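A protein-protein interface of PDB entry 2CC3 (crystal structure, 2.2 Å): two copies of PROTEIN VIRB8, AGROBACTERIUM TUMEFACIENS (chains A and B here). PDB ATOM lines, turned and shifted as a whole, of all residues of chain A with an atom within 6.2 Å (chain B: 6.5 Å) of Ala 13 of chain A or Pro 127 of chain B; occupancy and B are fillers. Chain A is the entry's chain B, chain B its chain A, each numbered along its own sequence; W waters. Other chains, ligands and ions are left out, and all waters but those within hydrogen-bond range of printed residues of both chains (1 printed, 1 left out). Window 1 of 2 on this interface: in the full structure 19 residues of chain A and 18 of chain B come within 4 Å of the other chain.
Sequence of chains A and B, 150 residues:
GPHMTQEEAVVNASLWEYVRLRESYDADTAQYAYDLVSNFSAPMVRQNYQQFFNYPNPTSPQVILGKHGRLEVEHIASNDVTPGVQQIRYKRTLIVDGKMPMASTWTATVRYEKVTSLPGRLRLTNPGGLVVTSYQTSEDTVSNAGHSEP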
ATOM      1  N   THR A   5       7.421  -3.352  22.646  1.00  0.00           N
ATOM      2  CA  THR A   5       8.015  -4.210  21.623  1.00  0.00           C
ATOM      3  C   THR A   5       9.045  -3.391  20.864  1.00  0.00           C
ATOM      4  O   THR A   5       8.929  -2.173  20.798  1.00  0.00           O
ATOM      5  CB  THR A   5       6.946  -4.809  20.659  1.00  0.00           C
ATOM      6  OG1 THR A   5       6.118  -3.759  20.145  1.00  0.00           O
ATOM      7  CG2 THR A   5       6.063  -5.820  21.399  1.00  0.00           C
ATOM      8  N   GLN A   6      10.065  -4.058  20.327  1.00  0.00           N
ATOM      9  CA  GLN A   6      11.067  -3.411  19.496  1.00  0.00           C
ATOM     10  C   GLN A   6      10.391  -2.741  18.276  1.00  0.00           C
ATOM     11  O   GLN A   6      10.723  -1.610  17.903  1.00  0.00           O
ATOM     12  CB  GLN A   6      12.130  -4.448  19.085  1.00  0.00           C
ATOM     13  CG  GLN A   6      13.596  -4.017  19.321  1.00  0.00           C
ATOM     14  CD  GLN A   6      14.379  -3.709  18.041  1.00  0.00           C
ATOM     15  OE1 GLN A   6      15.169  -4.518  17.577  1.00  0.00           O
ATOM     16  NE2 GLN A   6      14.169  -2.536  17.489  1.00  0.00           N
ATOM     17  N   GLU A   8       7.309  -1.476  17.935  1.00  0.00           N
ATOM     18  CA  GLU A   8       6.701  -0.279  18.489  1.00  0.00           C
ATOM     19  C   GLU A   8       7.757   0.811  18.753  1.00  0.00           C
ATOM     20  O   GLU A   8       7.532   1.983  18.498  1.00  0.00           O
ATOM     21  CB  GLU A   8       6.105  -0.722  19.819  1.00  0.00           C
ATOM     22  CG  GLU A   8       4.802  -0.139  20.275  1.00  0.00           C
ATOM     23  CD  GLU A   8       4.302  -0.883  21.504  1.00  0.00           C
ATOM     24  OE1 GLU A   8       4.307  -2.133  21.486  1.00  0.00           O
ATOM     25  OE2 GLU A   8       3.927  -0.232  22.500  1.00  0.00           O
ATOM     26  N   ALA A   9       8.906   0.411  19.297  1.00  0.00           N
ATOM     27  CA  ALA A   9      10.038   1.308  19.508  1.00  0.00           C
ATOM     28  C   ALA A   9      10.591   1.887  18.179  1.00  0.00           C
ATOM     29  O   ALA A   9      10.896   3.075  18.070  1.00  0.00           O
ATOM     30  CB  ALA A   9      11.130   0.553  20.284  1.00  0.00           C
ATOM     31  N   VAL A  10      10.777   1.022  17.200  1.00  0.00           N
ATOM     32  CA  VAL A  10      11.202   1.414  15.862  1.00  0.00           C
ATOM     33  C   VAL A  10      10.206   2.384  15.172  1.00  0.00           C
ATOM     34  O   VAL A  10      10.629   3.382  14.592  1.00  0.00           O
ATOM     35  CB  VAL A  10      11.526   0.145  14.998  1.00  0.00           C
ATOM     36  CG1 VAL A  10      11.786   0.500  13.532  1.00  0.00           C
ATOM     37  CG2 VAL A  10      12.774  -0.545  15.550  1.00  0.00           C
ATOM     38  N   VAL A  11       8.910   2.114  15.267  1.00  0.00           N
ATOM     39  CA  VAL A  11       7.866   3.026  14.740  1.00  0.00           C
ATOM     40  C   VAL A  11       7.997   4.430  15.296  1.00  0.00           C
ATOM     41  O   VAL A  11       8.048   5.400  14.545  1.00  0.00           O
ATOM     42  CB  VAL A  11       6.442   2.511  15.053  1.00  0.00           C
ATOM     43  CG1 VAL A  11       5.410   3.529  14.616  1.00  0.00           C
ATOM     44  CG2 VAL A  11       6.165   1.194  14.321  1.00  0.00           C
ATOM     45  N   ASN A  12       8.089   4.512  16.634  1.00  0.00           N
ATOM     46  CA  ASN A  12       8.072   5.755  17.396  1.00  0.00           C
ATOM     47  C   ASN A  12       9.289   6.609  17.073  1.00  0.00           C
ATOM     48  O   ASN A  12       9.200   7.836  16.944  1.00  0.00           O
ATOM     49  CB  ASN A  12       8.064   5.428  18.910  1.00  0.00           C
ATOM     50  CG  ASN A  12       6.749   4.806  19.409  1.00  0.00           C
ATOM     51  OD1 ASN A  12       5.673   5.045  18.873  1.00  0.00           O
ATOM     52  ND2 ASN A  12       6.846   4.026  20.473  1.00  0.00           N
ATOM     53  N   ALA A  13      10.438   5.932  17.001  1.00  0.00           N
ATOM     54  CA  ALA A  13      11.730   6.521  16.626  1.00  0.00           C
ATOM     55  C   ALA A  13      11.721   7.073  15.211  1.00  0.00           C
ATOM     56  O   ALA A  13      12.196   8.189  14.978  1.00  0.00           O
ATOM     57  CB  ALA A  13      12.865   5.489  16.786  1.00  0.00           C
ATOM     58  N   SER A  14      11.206   6.287  14.283  1.00  0.00           N
ATOM     59  CA  SER A  14      11.202   6.618  12.834  1.00  0.00           C
ATOM     60  C   SER A  14      10.256   7.802  12.514  1.00  0.00           C
ATOM     61  O   SER A  14      10.636   8.731  11.778  1.00  0.00           O
ATOM     62  CB  SER A  14      10.758   5.387  12.016  1.00  0.00           C
ATOM     63  OG  SER A  14      11.670   4.294  12.068  1.00  0.00           O
ATOM     64  N   LEU A  15       9.046   7.760  13.071  1.00  0.00           N
ATOM     65  CA  LEU A  15       8.031   8.845  12.907  1.00  0.00           C
ATOM     66  C   LEU A  15       8.453  10.167  13.518  1.00  0.00           C
ATOM     67  O   LEU A  15       8.214  11.236  12.930  1.00  0.00           O
ATOM     68  CB  LEU A  15       6.682   8.430  13.486  1.00  0.00           C
ATOM     69  CG  LEU A  15       6.038   7.210  12.819  1.00  0.00           C
ATOM     70  CD1 LEU A  15       4.729   6.852  13.506  1.00  0.00           C
ATOM     71  CD2 LEU A  15       5.848   7.458  11.309  1.00  0.00           C
ATOM     72  N   TRP A  16       9.095  10.090  14.687  1.00  0.00           N
ATOM     73  CA  TRP A  16       9.692  11.257  15.336  1.00  0.00           C
ATOM     74  C   TRP A  16      10.882  11.831  14.563  1.00  0.00           C
ATOM     75  O   TRP A  16      11.008  13.059  14.377  1.00  0.00           O
ATOM     76  CB  TRP A  16      10.106  10.927  16.796  1.00  0.00           C
ATOM     77  CG  TRP A  16      10.959  12.039  17.298  1.00  0.00           C
ATOM     78  CD1 TRP A  16      12.292  11.993  17.589  1.00  0.00           C
ATOM     79  CD2 TRP A  16      10.555  13.395  17.463  1.00  0.00           C
ATOM     80  NE1 TRP A  16      12.736  13.242  17.955  1.00  0.00           N
ATOM     81  CE2 TRP A  16      11.687  14.122  17.879  1.00  0.00           C
ATOM     82  CE3 TRP A  16       9.335  14.072  17.298  1.00  0.00           C
ATOM     83  CZ2 TRP A  16      11.638  15.487  18.136  1.00  0.00           C
ATOM     84  CZ3 TRP A  16       9.293  15.438  17.543  1.00  0.00           C
ATOM     85  CH2 TRP A  16      10.424  16.124  17.963  1.00  0.00           C
ATOM     86  N   GLU A  17      11.784  10.960  14.124  1.00  0.00           N
ATOM     87  CA  GLU A  17      12.800  11.396  13.150  1.00  0.00           C
ATOM     88  C   GLU A  17      12.128  12.075  11.948  1.00  0.00           C
ATOM     89  O   GLU A  17      12.567  13.162  11.519  1.00  0.00           O
ATOM     90  CB  GLU A  17      13.708  10.244  12.694  1.00  0.00           C
ATOM     91  CG  GLU A  17      15.078  10.734  12.219  1.00  0.00           C
ATOM     92  CD  GLU A  17      15.732   9.823  11.182  1.00  0.00           C
ATOM     93  OE1 GLU A  17      15.425   8.607  11.144  1.00  0.00           O
ATOM     94  OE2 GLU A  17      16.580  10.309  10.400  1.00  0.00           O
ATOM     95  N   TYR A  18      11.064  11.451  11.429  1.00  0.00           N
ATOM     96  CA  TYR A  18      10.295  12.015  10.303  1.00  0.00           C
ATOM     97  C   TYR A  18       9.850  13.453  10.633  1.00  0.00           C
ATOM     98  O   TYR A  18      10.216  14.414   9.924  1.00  0.00           O
ATOM     99  CB  TYR A  18       9.103  11.106   9.898  1.00  0.00           C
ATOM    100  CG  TYR A  18       8.392  11.627   8.654  1.00  0.00           C
ATOM    101  CD1 TYR A  18       8.907  11.378   7.365  1.00  0.00           C
ATOM    102  CD2 TYR A  18       7.240  12.421   8.771  1.00  0.00           C
ATOM    103  CE1 TYR A  18       8.259  11.912   6.207  1.00  0.00           C
ATOM    104  CE2 TYR A  18       6.593  12.924   7.669  1.00  0.00           C
ATOM    105  CZ  TYR A  18       7.099  12.685   6.386  1.00  0.00           C
ATOM    106  OH  TYR A  18       6.410  13.211   5.307  1.00  0.00           O
ATOM    107  N   VAL B  10      17.747  -2.884  12.300  1.00  0.00           N
ATOM    108  CA  VAL B  10      17.904  -1.897  13.358  1.00  0.00           C
ATOM    109  C   VAL B  10      19.357  -1.728  13.821  1.00  0.00           C
ATOM    110  O   VAL B  10      19.819  -0.595  14.005  1.00  0.00           O
ATOM    111  CB  VAL B  10      16.929  -2.206  14.518  1.00  0.00           C
ATOM    112  CG1 VAL B  10      17.043  -1.171  15.649  1.00  0.00           C
ATOM    113  CG2 VAL B  10      15.500  -2.198  13.971  1.00  0.00           C
ATOM    114  N   SER B  14      21.428   1.751  13.344  1.00  0.00           N
ATOM    115  CA  SER B  14      21.836   2.555  14.548  1.00  0.00           C
ATOM    116  C   SER B  14      23.378   2.751  14.576  1.00  0.00           C
ATOM    117  O   SER B  14      23.878   3.808  14.971  1.00  0.00           O
ATOM    118  CB  SER B  14      21.367   1.949  15.890  1.00  0.00           C
ATOM    119  OG  SER B  14      19.999   1.541  15.938  1.00  0.00           O
ATOM    120  N   PHE B  40      24.835   7.111  23.291  1.00  0.00           N
ATOM    121  CA  PHE B  40      24.988   5.809  22.663  1.00  0.00           C
ATOM    122  C   PHE B  40      26.245   5.022  23.141  1.00  0.00           C
ATOM    123  O   PHE B  40      26.389   3.844  22.828  1.00  0.00           O
ATOM    124  CB  PHE B  40      25.170   6.035  21.146  1.00  0.00           C
ATOM    125  CG  PHE B  40      23.911   5.851  20.299  1.00  0.00           C
ATOM    126  CD1 PHE B  40      23.140   6.955  19.902  1.00  0.00           C
ATOM    127  CD2 PHE B  40      23.550   4.594  19.818  1.00  0.00           C
ATOM    128  CE1 PHE B  40      21.984   6.802  19.082  1.00  0.00           C
ATOM    129  CE2 PHE B  40      22.401   4.428  19.000  1.00  0.00           C
ATOM    130  CZ  PHE B  40      21.626   5.535  18.633  1.00  0.00           C
ATOM    131  N   LEU B 118      16.008   1.665  28.724  1.00  0.00           N
ATOM    132  CA  LEU B 118      16.533   2.996  28.420  1.00  0.00           C
ATOM    133  C   LEU B 118      15.497   3.974  28.932  1.00  0.00           C
ATOM    134  O   LEU B 118      14.319   3.648  28.899  1.00  0.00           O
ATOM    135  CB  LEU B 118      16.706   3.193  26.913  1.00  0.00           C
ATOM    136  CG  LEU B 118      17.933   2.630  26.190  1.00  0.00           C
ATOM    137  CD1 LEU B 118      17.748   2.886  24.727  1.00  0.00           C
ATOM    138  CD2 LEU B 118      19.212   3.316  26.661  1.00  0.00           C
ATOM    139  N   LEU B 122      15.800   8.515  25.508  1.00  0.00           N
ATOM    140  CA  LEU B 122      16.807   7.729  24.805  1.00  0.00           C
ATOM    141  C   LEU B 122      16.217   6.612  23.936  1.00  0.00           C
ATOM    142  O   LEU B 122      16.639   6.400  22.830  1.00  0.00           O
ATOM    143  CB  LEU B 122      17.830   7.146  25.803  1.00  0.00           C
ATOM    144  CG  LEU B 122      19.044   7.988  26.213  1.00  0.00           C
ATOM    145  CD1 LEU B 122      18.672   9.202  26.945  1.00  0.00           C
ATOM    146  CD2 LEU B 122      20.023   7.196  27.068  1.00  0.00           C
ATOM    147  N   ARG B 123      15.229   5.905  24.455  1.00  0.00           N
ATOM    148  CA  ARG B 123      14.497   4.906  23.675  1.00  0.00           C
ATOM    149  C   ARG B 123      14.030   5.497  22.327  1.00  0.00           C
ATOM    150  O   ARG B 123      14.124   4.846  21.283  1.00  0.00           O
ATOM    151  CB  ARG B 123      13.293   4.396  24.502  1.00  0.00           C
ATOM    152  CG  ARG B 123      12.595   3.157  23.952  1.00  0.00           C
ATOM    153  CD  ARG B 123      13.582   2.052  23.639  1.00  0.00           C
ATOM    154  NE  ARG B 123      13.803   1.223  24.803  1.00  0.00           N
ATOM    155  CZ  ARG B 123      14.486   0.088  24.825  1.00  0.00           C
ATOM    156  NH1 ARG B 123      15.031  -0.374  23.715  1.00  0.00           N
ATOM    157  NH2 ARG B 123      14.604  -0.602  25.972  1.00  0.00           N
ATOM    158  N   LEU B 124      13.552   6.735  22.370  1.00  0.00           N
ATOM    159  CA  LEU B 124      13.070   7.471  21.188  1.00  0.00           C
ATOM    160  C   LEU B 124      14.073   7.583  20.006  1.00  0.00           C
ATOM    161  O   LEU B 124      13.667   7.707  18.865  1.00  0.00           O
ATOM    162  CB  LEU B 124      12.608   8.874  21.620  1.00  0.00           C
ATOM    163  CG  LEU B 124      11.842   9.764  20.645  1.00  0.00           C
ATOM    164  CD1 LEU B 124      10.403   9.262  20.385  1.00  0.00           C
ATOM    165  CD2 LEU B 124      11.844  11.162  21.154  1.00  0.00           C
ATOM    166  N   THR B 125      15.374   7.546  20.296  1.00  0.00           N
ATOM    167  CA  THR B 125      16.408   7.809  19.284  1.00  0.00           C
ATOM    168  C   THR B 125      17.292   6.556  19.098  1.00  0.00           C
ATOM    169  O   THR B 125      18.134   6.465  18.182  1.00  0.00           O
ATOM    170  CB  THR B 125      17.250   9.025  19.707  1.00  0.00           C
ATOM    171  OG1 THR B 125      17.838   8.774  20.978  1.00  0.00           O
ATOM    172  CG2 THR B 125      16.402  10.250  19.875  1.00  0.00           C
ATOM    173  N   ASN B 126      17.070   5.582  19.973  1.00  0.00           N
ATOM    174  CA  ASN B 126      17.848   4.337  20.040  1.00  0.00           C
ATOM    175  C   ASN B 126      16.814   3.264  20.409  1.00  0.00           C
ATOM    176  O   ASN B 126      16.835   2.751  21.528  1.00  0.00           O
ATOM    177  CB  ASN B 126      18.941   4.493  21.119  1.00  0.00           C
ATOM    178  CG  ASN B 126      19.880   3.319  21.219  1.00  0.00           C
ATOM    179  OD1 ASN B 126      19.911   2.422  20.359  1.00  0.00           O
ATOM    180  ND2 ASN B 126      20.697   3.324  22.274  1.00  0.00           N
ATOM    181  N   PRO B 127      15.878   2.960  19.488  1.00  0.00           N
ATOM    182  CA  PRO B 127      14.862   1.926  19.694  1.00  0.00           C
ATOM    183  C   PRO B 127      15.367   0.548  20.083  1.00  0.00           C
ATOM    184  O   PRO B 127      14.665  -0.172  20.800  1.00  0.00           O
ATOM    185  CB  PRO B 127      14.138   1.846  18.326  1.00  0.00           C
ATOM    186  CG  PRO B 127      15.061   2.599  17.324  1.00  0.00           C
ATOM    187  CD  PRO B 127      15.724   3.631  18.170  1.00  0.00           C
ATOM    188  N   GLY B 128      16.540   0.152  19.586  1.00  0.00           N
ATOM    189  CA  GLY B 128      17.074  -1.177  19.870  1.00  0.00           C
ATOM    190  C   GLY B 128      17.942  -1.318  21.125  1.00  0.00           C
ATOM    191  O   GLY B 128      18.404  -2.410  21.434  1.00  0.00           O
ATOM    192  N   GLY B 129      18.201  -0.223  21.819  1.00  0.00           N
ATOM    193  CA  GLY B 129      18.943  -0.274  23.076  1.00  0.00           C
ATOM    194  C   GLY B 129      20.431  -0.543  22.895  1.00  0.00           C
ATOM    195  O   GLY B 129      21.085  -1.100  23.771  1.00  0.00           O
ATOM    196  N   LEU B 130      20.966  -0.098  21.766  1.00  0.00           N
ATOM    197  CA  LEU B 130      22.361  -0.287  21.412  1.00  0.00           C
ATOM    198  C   LEU B 130      23.274   0.689  22.142  1.00  0.00           C
ATOM    199  O   LEU B 130      23.035   1.891  22.154  1.00  0.00           O
ATOM    200  CB  LEU B 130      22.561  -0.123  19.894  1.00  0.00           C
ATOM    201  CG  LEU B 130      21.964  -1.163  18.939  1.00  0.00           C
ATOM    202  CD1 LEU B 130      22.707  -1.123  17.606  1.00  0.00           C
ATOM    203  CD2 LEU B 130      22.006  -2.595  19.548  1.00  0.00           C
HETATM  204  O   HOH W   1      11.461   4.492  20.276  1.00  0.00           O
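The backbone carbonyl oxygen (O) of Val 10 of chain B sits at hydrogen-bond distance from the side-chain hydroxyl (OG) of Ser 14 of chain B, at 2.9 Å. The backbone carbonyl oxygen (O) of Pro 127 of chain B lies within hydrogen-bond range of the guanidinium group (NH1) of Arg 123 of chain B, 2.9 Å away. ND2 of Asn 12 of chain A sits at hydrogen-bond distance from O of Glu 8 of chain A (2.9 Å). OG of Ser 14 of chain A sits at hydrogen-bond distance from O of Val 10 of chain A (2.9 Å).
Among the printed residues, pairs that only touch across the chains: Ala 13 of chain A with Leu 124 of chain B, Ala 9 of chain A with Pro 127 of chain B, Val 10 of chain A with Val 10 of chain B, Val 10 of chain A with Pro 127 of chain B, Ala 13 of chain A with Pro 127 of chain B, Gln 6 of chain A with Val 10 of chain B, Trp 16 of chain A with Leu 124 of chain B, Asn 12 of chain A with Leu 124 of chain B and Gln 6 of chain A with Gly 128 of chain B.
Water W1 lies within hydrogen-bond range of O of Ala 9 of chain A (2.7 Å) and O of Arg 123 of chain B (2.9 Å).
Of the 13 printed residues of chain A, 6 touch a printed residue of chain B. Hydrophobic or aromatic side chains of chain A that line the printed part of chain B: Ala 9, Val 10, Ala 13 and Trp 16. Along chain A the printed residues that touch a printed residue of chain B span positions 6 to 16. Among the printed residues, 9 pairs touch across the chains.
Val 10 of chain A touches its own counterpart, Val 10 of chain B.
Ala 13 of chain A touches just these residues of chain B: Leu 124 (3.1 Å) and Pro 127 (3.7 Å). Pro 127 of chain B touches just these residues of chain A: Ala 9, Val 10 and Ala 13. Of the printed residues of chain B, Asn 12 of chain A touches Leu 124 (3.9 Å). Printed residues of chain B within 4 Å of Gln 6 of chain A: Val 10 (3.7 Å) and Gly 128 (3.99 Å). Of the printed residues of chain A, Val 10 of chain B touches Gln 6 and Val 10. Of the printed residues of chain A, Leu 124 of chain B touches Asn 12, Ala 13 and Trp 16. Leu 118 of chain B touches none of the printed residues of chain A.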
